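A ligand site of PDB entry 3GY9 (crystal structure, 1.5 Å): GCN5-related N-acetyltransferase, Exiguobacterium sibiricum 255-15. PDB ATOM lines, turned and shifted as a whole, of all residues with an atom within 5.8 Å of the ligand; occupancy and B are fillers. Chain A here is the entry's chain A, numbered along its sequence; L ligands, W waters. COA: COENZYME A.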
ATOM      1  N   GLU A  27       3.372   6.757  -3.157  1.00  0.00           N
ATOM      2  CA  GLU A  27       4.115   7.977  -3.428  1.00  0.00           C
ATOM      3  C   GLU A  27       3.451   8.913  -4.424  1.00  0.00           C
ATOM      4  O   GLU A  27       3.959  10.003  -4.666  1.00  0.00           O
ATOM      5  CB  GLU A  27       5.502   7.619  -3.938  1.00  0.00           C
ATOM      6  CG  GLU A  27       6.400   7.073  -2.887  1.00  0.00           C
ATOM      7  CD  GLU A  27       7.801   6.948  -3.381  1.00  0.00           C
ATOM      8  OE1 GLU A  27       7.961   6.373  -4.468  1.00  0.00           O
ATOM      9  OE2 GLU A  27       8.730   7.424  -2.683  1.00  0.00           O
ATOM     10  N   PHE A  29       2.806   7.988  -7.703  1.00  0.00           N
ATOM     11  CA  PHE A  29       3.306   7.702  -9.054  1.00  0.00           C
ATOM     12  C   PHE A  29       2.401   6.669  -9.718  1.00  0.00           C
ATOM     13  O   PHE A  29       2.052   5.655  -9.107  1.00  0.00           O
ATOM     14  CB  PHE A  29       4.724   7.121  -9.020  1.00  0.00           C
ATOM     15  CG  PHE A  29       5.795   8.096  -8.612  1.00  0.00           C
ATOM     16  CD1 PHE A  29       6.093   9.198  -9.403  1.00  0.00           C
ATOM     17  CD2 PHE A  29       6.528   7.903  -7.447  1.00  0.00           C
ATOM     18  CE1 PHE A  29       7.093  10.101  -9.025  1.00  0.00           C
ATOM     19  CE2 PHE A  29       7.521   8.779  -7.083  1.00  0.00           C
ATOM     20  CZ  PHE A  29       7.803   9.889  -7.860  1.00  0.00           C
ATOM     21  N   VAL A  82      10.818   4.135 -15.139  1.00  0.00           N
ATOM     22  CA  VAL A  82      11.920   3.880 -14.231  1.00  0.00           C
ATOM     23  C   VAL A  82      11.490   4.166 -12.809  1.00  0.00           C
ATOM     24  O   VAL A  82      11.062   5.268 -12.498  1.00  0.00           O
ATOM     25  CB  VAL A  82      13.129   4.784 -14.569  1.00  0.00           C
ATOM     26  CG1 VAL A  82      14.180   4.699 -13.465  1.00  0.00           C
ATOM     27  CG2 VAL A  82      13.695   4.414 -15.927  1.00  0.00           C
ATOM     28  N   TYR A  83      11.592   3.169 -11.952  1.00  0.00           N
ATOM     29  CA  TYR A  83      11.163   3.292 -10.547  1.00  0.00           C
ATOM     30  C   TYR A  83      11.953   2.320  -9.692  1.00  0.00           C
ATOM     31  O   TYR A  83      12.080   1.146 -10.044  1.00  0.00           O
ATOM     32  CB  TYR A  83       9.665   2.973 -10.413  1.00  0.00           C
ATOM     33  CG  TYR A  83       9.169   3.165  -9.002  1.00  0.00           C
ATOM     34  CD1 TYR A  83       8.852   4.431  -8.519  1.00  0.00           C
ATOM     35  CD2 TYR A  83       9.033   2.084  -8.158  1.00  0.00           C
ATOM     36  CE1 TYR A  83       8.411   4.600  -7.213  1.00  0.00           C
ATOM     37  CE2 TYR A  83       8.595   2.259  -6.845  1.00  0.00           C
ATOM     38  CZ  TYR A  83       8.291   3.510  -6.383  1.00  0.00           C
ATOM     39  OH  TYR A  83       7.849   3.700  -5.083  1.00  0.00           O
ATOM     40  N   VAL A  84      12.506   2.818  -8.577  1.00  0.00           N
ATOM     41  CA  VAL A  84      13.211   1.979  -7.607  1.00  0.00           C
ATOM     42  C   VAL A  84      12.426   2.029  -6.306  1.00  0.00           C
ATOM     43  O   VAL A  84      12.009   3.113  -5.879  1.00  0.00           O
ATOM     44  CB  VAL A  84      14.635   2.507  -7.336  1.00  0.00           C
ATOM     45  CG1 VAL A  84      15.367   1.656  -6.293  1.00  0.00           C
ATOM     46  CG2 VAL A  84      15.415   2.536  -8.638  1.00  0.00           C
ATOM     47  N   LEU A  85      12.197   0.876  -5.688  1.00  0.00           N
ATOM     48  CA  LEU A  85      11.499   0.812  -4.389  1.00  0.00           C
ATOM     49  C   LEU A  85      12.188   1.735  -3.400  1.00  0.00           C
ATOM     50  O   LEU A  85      13.418   1.767  -3.335  1.00  0.00           O
ATOM     51  CB  LEU A  85      11.498  -0.602  -3.798  1.00  0.00           C
ATOM     52  CG  LEU A  85      10.536  -1.660  -4.351  1.00  0.00           C
ATOM     53  CD1 LEU A  85      10.805  -2.960  -3.613  1.00  0.00           C
ATOM     54  CD2 LEU A  85       9.081  -1.238  -4.198  1.00  0.00           C
ATOM     55  N   PRO A  86      11.395   2.509  -2.629  1.00  0.00           N
ATOM     56  CA  PRO A  86      11.999   3.454  -1.697  1.00  0.00           C
ATOM     57  C   PRO A  86      13.115   2.873  -0.829  1.00  0.00           C
ATOM     58  O   PRO A  86      14.184   3.486  -0.714  1.00  0.00           O
ATOM     59  CB  PRO A  86      10.801   3.929  -0.858  1.00  0.00           C
ATOM     60  CG  PRO A  86       9.660   3.848  -1.800  1.00  0.00           C
ATOM     61  CD  PRO A  86       9.909   2.611  -2.604  1.00  0.00           C
ATOM     62  N   ALA A  88      15.139   0.557  -1.378  1.00  0.00           N
ATOM     63  CA  ALA A  88      16.268   0.088  -2.175  1.00  0.00           C
ATOM     64  C   ALA A  88      17.019   1.204  -2.879  1.00  0.00           C
ATOM     65  O   ALA A  88      17.981   0.939  -3.593  1.00  0.00           O
ATOM     66  CB  ALA A  88      15.818  -0.933  -3.193  1.00  0.00           C
ATOM     67  N   ARG A  89      16.579   2.445  -2.684  1.00  0.00           N
ATOM     68  CA  ARG A  89      17.247   3.608  -3.279  1.00  0.00           C
ATOM     69  C   ARG A  89      18.599   3.885  -2.639  1.00  0.00           C
ATOM     70  O   ARG A  89      18.886   3.419  -1.518  1.00  0.00           O
ATOM     71  CB  ARG A  89      16.359   4.827  -3.180  1.00  0.00           C
ATOM     72  CG  ARG A  89      15.133   4.702  -4.055  1.00  0.00           C
ATOM     73  CD  ARG A  89      14.130   5.798  -3.784  1.00  0.00           C
ATOM     74  NE  ARG A  89      12.907   5.441  -4.492  1.00  0.00           N
ATOM     75  CZ  ARG A  89      11.713   5.966  -4.266  1.00  0.00           C
ATOM     76  NH1 ARG A  89      11.526   6.911  -3.351  1.00  0.00           N
ATOM     77  NH2 ARG A  89      10.680   5.522  -4.990  1.00  0.00           N
ATOM     78  N   SER A  90      19.438   4.611  -3.370  1.00  0.00           N
ATOM     79  CA  SER A  90      20.727   5.124  -2.889  1.00  0.00           C
ATOM     80  C   SER A  90      21.760   4.006  -2.711  1.00  0.00           C
ATOM     81  O   SER A  90      22.687   4.152  -1.896  1.00  0.00           O
ATOM     82  CB  SER A  90      20.568   5.900  -1.587  1.00  0.00           C
ATOM     83  OG  SER A  90      19.608   6.925  -1.722  1.00  0.00           O
ATOM     84  N   HIS A  91      21.596   2.910  -3.448  1.00  0.00           N
ATOM     85  CA  HIS A  91      22.519   1.763  -3.412  1.00  0.00           C
ATOM     86  C   HIS A  91      23.030   1.370  -4.796  1.00  0.00           C
ATOM     87  O   HIS A  91      23.527   0.259  -4.982  1.00  0.00           O
ATOM     88  CB  HIS A  91      21.837   0.543  -2.785  1.00  0.00           C
ATOM     89  CG  HIS A  91      21.604   0.683  -1.325  1.00  0.00           C
ATOM     90  ND1 HIS A  91      20.356   0.900  -0.786  1.00  0.00           N
ATOM     91  CD2 HIS A  91      22.475   0.672  -0.285  1.00  0.00           C
ATOM     92  CE1 HIS A  91      20.464   1.006   0.536  1.00  0.00           C
ATOM     93  NE2 HIS A  91      21.737   0.878   0.855  1.00  0.00           N
ATOM     94  N   GLY A  92      22.873   2.267  -5.751  1.00  0.00           N
ATOM     95  CA  GLY A  92      23.424   2.076  -7.101  1.00  0.00           C
ATOM     96  C   GLY A  92      22.552   1.325  -8.071  1.00  0.00           C
ATOM     97  O   GLY A  92      22.949   1.085  -9.198  1.00  0.00           O
ATOM     98  N   ILE A  93      21.348   0.931  -7.660  1.00  0.00           N
ATOM     99  CA  ILE A  93      20.449   0.181  -8.560  1.00  0.00           C
ATOM    100  C   ILE A  93      19.998   1.018  -9.763  1.00  0.00           C
ATOM    101  O   ILE A  93      20.058   0.552 -10.912  1.00  0.00           O
ATOM    102  CB  ILE A  93      19.236  -0.365  -7.775  1.00  0.00           C
ATOM    103  CG1 ILE A  93      19.715  -1.365  -6.690  1.00  0.00           C
ATOM    104  CG2 ILE A  93      18.233  -1.026  -8.713  1.00  0.00           C
ATOM    105  CD1 ILE A  93      18.620  -1.755  -5.714  1.00  0.00           C
ATOM    106  N   GLY A  94      19.511   2.226  -9.515  1.00  0.00           N
ATOM    107  CA  GLY A  94      19.063   3.081 -10.605  1.00  0.00           C
ATOM    108  C   GLY A  94      20.178   3.307 -11.606  1.00  0.00           C
ATOM    109  O   GLY A  94      19.962   3.293 -12.835  1.00  0.00           O
ATOM    110  N   THR A  95      21.385   3.565 -11.117  1.00  0.00           N
ATOM    111  CA  THR A  95      22.518   3.743 -12.006  1.00  0.00           C
ATOM    112  C   THR A  95      22.755   2.516 -12.873  1.00  0.00           C
ATOM    113  O   THR A  95      22.913   2.654 -14.084  1.00  0.00           O
ATOM    114  CB  THR A  95      23.771   4.139 -11.231  1.00  0.00           C
ATOM    115  OG1 THR A  95      23.524   5.372 -10.558  1.00  0.00           O
ATOM    116  CG2 THR A  95      24.949   4.315 -12.169  1.00  0.00           C
ATOM    117  N   ALA A  96      22.752   1.323 -12.275  1.00  0.00           N
ATOM    118  CA  ALA A  96      23.009   0.112 -13.035  1.00  0.00           C
ATOM    119  C   ALA A  96      21.916  -0.120 -14.073  1.00  0.00           C
ATOM    120  O   ALA A  96      22.181  -0.505 -15.204  1.00  0.00           O
ATOM    121  CB  ALA A  96      23.082  -1.089 -12.126  1.00  0.00           C
ATOM    122  N   GLN A 118      11.062  14.637 -10.939  1.00  0.00           N
ATOM    123  CA  GLN A 118      11.588  14.499  -9.571  1.00  0.00           C
ATOM    124  C   GLN A 118      13.061  14.111  -9.487  1.00  0.00           C
ATOM    125  O   GLN A 118      13.636  14.211  -8.404  1.00  0.00           O
ATOM    126  CB  GLN A 118      10.747  13.473  -8.782  1.00  0.00           C
ATOM    127  CG  GLN A 118       9.254  13.781  -8.734  1.00  0.00           C
ATOM    128  N   ALA A 119      13.683  13.701 -10.580  1.00  0.00           N
ATOM    129  CA  ALA A 119      15.038  13.160 -10.467  1.00  0.00           C
ATOM    130  C   ALA A 119      16.059  13.804 -11.408  1.00  0.00           C
ATOM    131  O   ALA A 119      16.849  13.105 -12.060  1.00  0.00           O
ATOM    132  CB  ALA A 119      14.993  11.657 -10.668  1.00  0.00           C
ATOM    133  N   PRO A 121      18.903  15.610 -10.745  1.00  0.00           N
ATOM    134  CA  PRO A 121      20.303  15.322 -10.400  1.00  0.00           C
ATOM    135  C   PRO A 121      20.774  13.929 -10.873  1.00  0.00           C
ATOM    136  O   PRO A 121      21.879  13.811 -11.413  1.00  0.00           O
ATOM    137  CB  PRO A 121      20.291  15.384  -8.877  1.00  0.00           C
ATOM    138  CG  PRO A 121      19.197  16.367  -8.570  1.00  0.00           C
ATOM    139  CD  PRO A 121      18.136  16.038  -9.558  1.00  0.00           C
ATOM    140  N   PHE A 122      19.931  12.933 -10.657  1.00  0.00           N
ATOM    141  CA  PHE A 122      20.226  11.570 -11.122  1.00  0.00           C
ATOM    142  C   PHE A 122      20.496  11.563 -12.626  1.00  0.00           C
ATOM    143  O   PHE A 122      21.541  11.064 -13.075  1.00  0.00           O
ATOM    144  CB  PHE A 122      19.055  10.642 -10.793  1.00  0.00           C
ATOM    145  CG  PHE A 122      19.160   9.256 -11.384  1.00  0.00           C
ATOM    146  CD1 PHE A 122      20.228   8.430 -11.065  1.00  0.00           C
ATOM    147  CD2 PHE A 122      18.180   8.775 -12.244  1.00  0.00           C
ATOM    148  CE1 PHE A 122      20.317   7.150 -11.606  1.00  0.00           C
ATOM    149  CE2 PHE A 122      18.259   7.503 -12.758  1.00  0.00           C
ATOM    150  CZ  PHE A 122      19.349   6.696 -12.440  1.00  0.00           C
ATOM    151  N   TYR A 123      19.575  12.125 -13.403  1.00  0.00           N
ATOM    152  CA  TYR A 123      19.718  12.079 -14.868  1.00  0.00           C
ATOM    153  C   TYR A 123      20.863  12.943 -15.389  1.00  0.00           C
ATOM    154  O   TYR A 123      21.559  12.544 -16.320  1.00  0.00           O
ATOM    155  CB  TYR A 123      18.369  12.379 -15.558  1.00  0.00           C
ATOM    156  CG  TYR A 123      17.395  11.238 -15.346  1.00  0.00           C
ATOM    157  CD1 TYR A 123      17.645   9.995 -15.924  1.00  0.00           C
ATOM    158  CD2 TYR A 123      16.246  11.369 -14.562  1.00  0.00           C
ATOM    159  CE1 TYR A 123      16.799   8.929 -15.756  1.00  0.00           C
ATOM    160  CE2 TYR A 123      15.380  10.290 -14.387  1.00  0.00           C
ATOM    161  CZ  TYR A 123      15.670   9.072 -14.978  1.00  0.00           C
ATOM    162  OH  TYR A 123      14.864   7.954 -14.836  1.00  0.00           O
HETATM  163  N1A COA L   1      15.773   9.674  -4.407  1.00  0.00           N
HETATM  164  C2A COA L   1      16.044  10.362  -5.575  1.00  0.00           C
HETATM  165  N3A COA L   1      17.311  10.371  -6.109  1.00  0.00           N
HETATM  166  C4A COA L   1      18.305   9.699  -5.481  1.00  0.00           C
HETATM  167  C5A COA L   1      18.057   8.995  -4.307  1.00  0.00           C
HETATM  168  C6A COA L   1      16.782   8.980  -3.763  1.00  0.00           C
HETATM  169  N6A COA L   1      16.534   8.411  -2.589  1.00  0.00           N
HETATM  170  N7A COA L   1      19.228   8.435  -3.913  1.00  0.00           N
HETATM  171  C8A COA L   1      20.198   8.756  -4.808  1.00  0.00           C
HETATM  172  N9A COA L   1      19.632   9.554  -5.773  1.00  0.00           N
HETATM  173  C1B COA L   1      20.292  10.172  -6.919  1.00  0.00           C
HETATM  174  C2B COA L   1      21.604  10.849  -6.522  1.00  0.00           C
HETATM  175  O2B COA L   1      21.782  12.010  -7.301  1.00  0.00           O
HETATM  176  C3B COA L   1      22.638   9.808  -6.862  1.00  0.00           C
HETATM  177  O3B COA L   1      23.906  10.350  -7.167  1.00  0.00           O
HETATM  178  P3B COA L   1      25.096  10.105  -6.118  1.00  0.00           P
HETATM  179  O7A COA L   1      26.366  10.738  -6.632  1.00  0.00           O
HETATM  180  O8A COA L   1      24.669  10.713  -4.807  1.00  0.00           O
HETATM  181  O9A COA L   1      25.324   8.624  -5.921  1.00  0.00           O
HETATM  182  C4B COA L   1      22.031   9.161  -8.086  1.00  0.00           C
HETATM  183  O4B COA L   1      20.627   9.165  -7.856  1.00  0.00           O
HETATM  184  C5B COA L   1      22.552   7.751  -8.344  1.00  0.00           C
HETATM  185  O5B COA L   1      22.319   6.941  -7.220  1.00  0.00           O
HETATM  186  P1A COA L   1      21.639   5.469  -7.321  1.00  0.00           P
HETATM  187  O1A COA L   1      22.175   4.685  -8.480  1.00  0.00           O
HETATM  188  O2A COA L   1      21.852   4.870  -5.975  1.00  0.00           O
HETATM  189  O3A COA L   1      20.111   5.907  -7.503  1.00  0.00           O
HETATM  190  P2A COA L   1      18.795   5.090  -7.127  1.00  0.00           P
HETATM  191  O4A COA L   1      19.008   3.581  -7.160  1.00  0.00           O
HETATM  192  O5A COA L   1      18.207   5.657  -5.893  1.00  0.00           O
HETATM  193  O6A COA L   1      17.878   5.465  -8.386  1.00  0.00           O
HETATM  194  CBP COA L   1      16.027   6.961  -8.867  1.00  0.00           C
HETATM  195  CCP COA L   1      17.540   6.823  -8.677  1.00  0.00           C
HETATM  196  CDP COA L   1      15.617   6.162 -10.107  1.00  0.00           C
HETATM  197  CEP COA L   1      15.717   8.457  -9.086  1.00  0.00           C
HETATM  198  CAP COA L   1      15.289   6.405  -7.628  1.00  0.00           C
HETATM  199  OAP COA L   1      15.794   7.034  -6.472  1.00  0.00           O
HETATM  200  C9P COA L   1      13.811   6.658  -7.725  1.00  0.00           C
HETATM  201  O9P COA L   1      12.966   5.792  -8.433  1.00  0.00           O
HETATM  202  N8P COA L   1      13.393   7.759  -7.108  1.00  0.00           N
HETATM  203  C7P COA L   1      11.988   8.152  -7.097  1.00  0.00           C
HETATM  204  C6P COA L   1      11.826   9.673  -7.158  1.00  0.00           C
HETATM  205  C5P COA L   1      12.341  10.305  -5.892  1.00  0.00           C
HETATM  206  O5P COA L   1      13.091   9.666  -5.124  1.00  0.00           O
HETATM  207  N4P COA L   1      11.962  11.561  -5.651  1.00  0.00           N
HETATM  208  C3P COA L   1      12.595  12.389  -4.646  1.00  0.00           C
HETATM  209  C2P COA L   1      12.286  11.918  -3.231  1.00  0.00           C
HETATM  210  S1P COA L   1      10.518  11.801  -2.832  1.00  0.00           S
HETATM  211  O   HOH W   1      23.666   8.041  -3.773  1.00  0.00           O
HETATM  212  O   HOH W   2      17.918  12.767  -8.342  1.00  0.00           O
HETATM  213  O   HOH W   3      24.017   5.645  -4.608  1.00  0.00           O
HETATM  214  O   HOH W   4      24.512  11.939  -9.743  1.00  0.00           O
HETATM  215  O   HOH W   5      19.784   1.904  -5.357  1.00  0.00           O
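The side-chain hydroxyl (OG) of Ser 90 lies within hydrogen-bond range of a nitrogen (N7A) of the ligand.
The side-chain hydroxyl (OG1) of Thr 95 lies within hydrogen-bond range of an oxygen (O1A) of the ligand (2.6 Å).
O2A of the ligand lies within hydrogen-bond range of N of Gly 92 (2.8 Å).
An oxygen (O2A) of the ligand is in hydrogen-bond range of the backbone NH (N) of His 91, at 3.2 Å.
The backbone NH of Val 84 lies within hydrogen-bond range of an oxygen (O9P) of the ligand (3.0 Å).
An oxygen (O1A) of the ligand is in hydrogen-bond range of the backbone NH (N) of Thr 95.
N of Gly 94 is in hydrogen-bond range of O4A of the ligand (2.8 Å).
The backbone NH (N) of Ser 90 sits at hydrogen-bond distance from an oxygen (O5A) of the ligand, 3.0 Å away.
Merely in contact with the ligand: Phe 122 (3.3 Å), Arg 89 (3.4 Å), Ile 93 (3.6 Å), Ala 119 (3.6 Å), Tyr 83 (3.7 Å), Gln 118 (3.9 Å) and Val 82 (3.9 Å).
Hydrophobic or aromatic side chains within 4 Å of the ligand: Val 82, Val 84, Ala 119 and Phe 122.
Water W3 lies within hydrogen-bond range of an oxygen (O2A) of the ligand (2.7 Å) and the backbone carbonyl oxygen (O) of Ser 90 (3.4 Å).
Water W2 lies within hydrogen-bond range of the backbone NH (N) of Phe 122 (3.1 Å) and a nitrogen (N3A) of the ligand (3.3 Å).
The side-chain hydroxyl of Tyr 83 is in hydrogen-bond range of the side-chain carboxylate of Glu 27, at 2.7 Å.
NH2 of Arg 89 lies within salt-bridge range of OE1 of Glu 27 (2.9 Å).
The guanidinium group (NH2) of Arg 89 lies close to the side-chain hydroxyl (OH) of Tyr 83 (3.4 Å).
ND1 of His 91 lies within hydrogen-bond range of O of Arg 89 (3.0 Å).
NE of Arg 89 is in hydrogen-bond range of O of Val 84 (2.9 Å).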
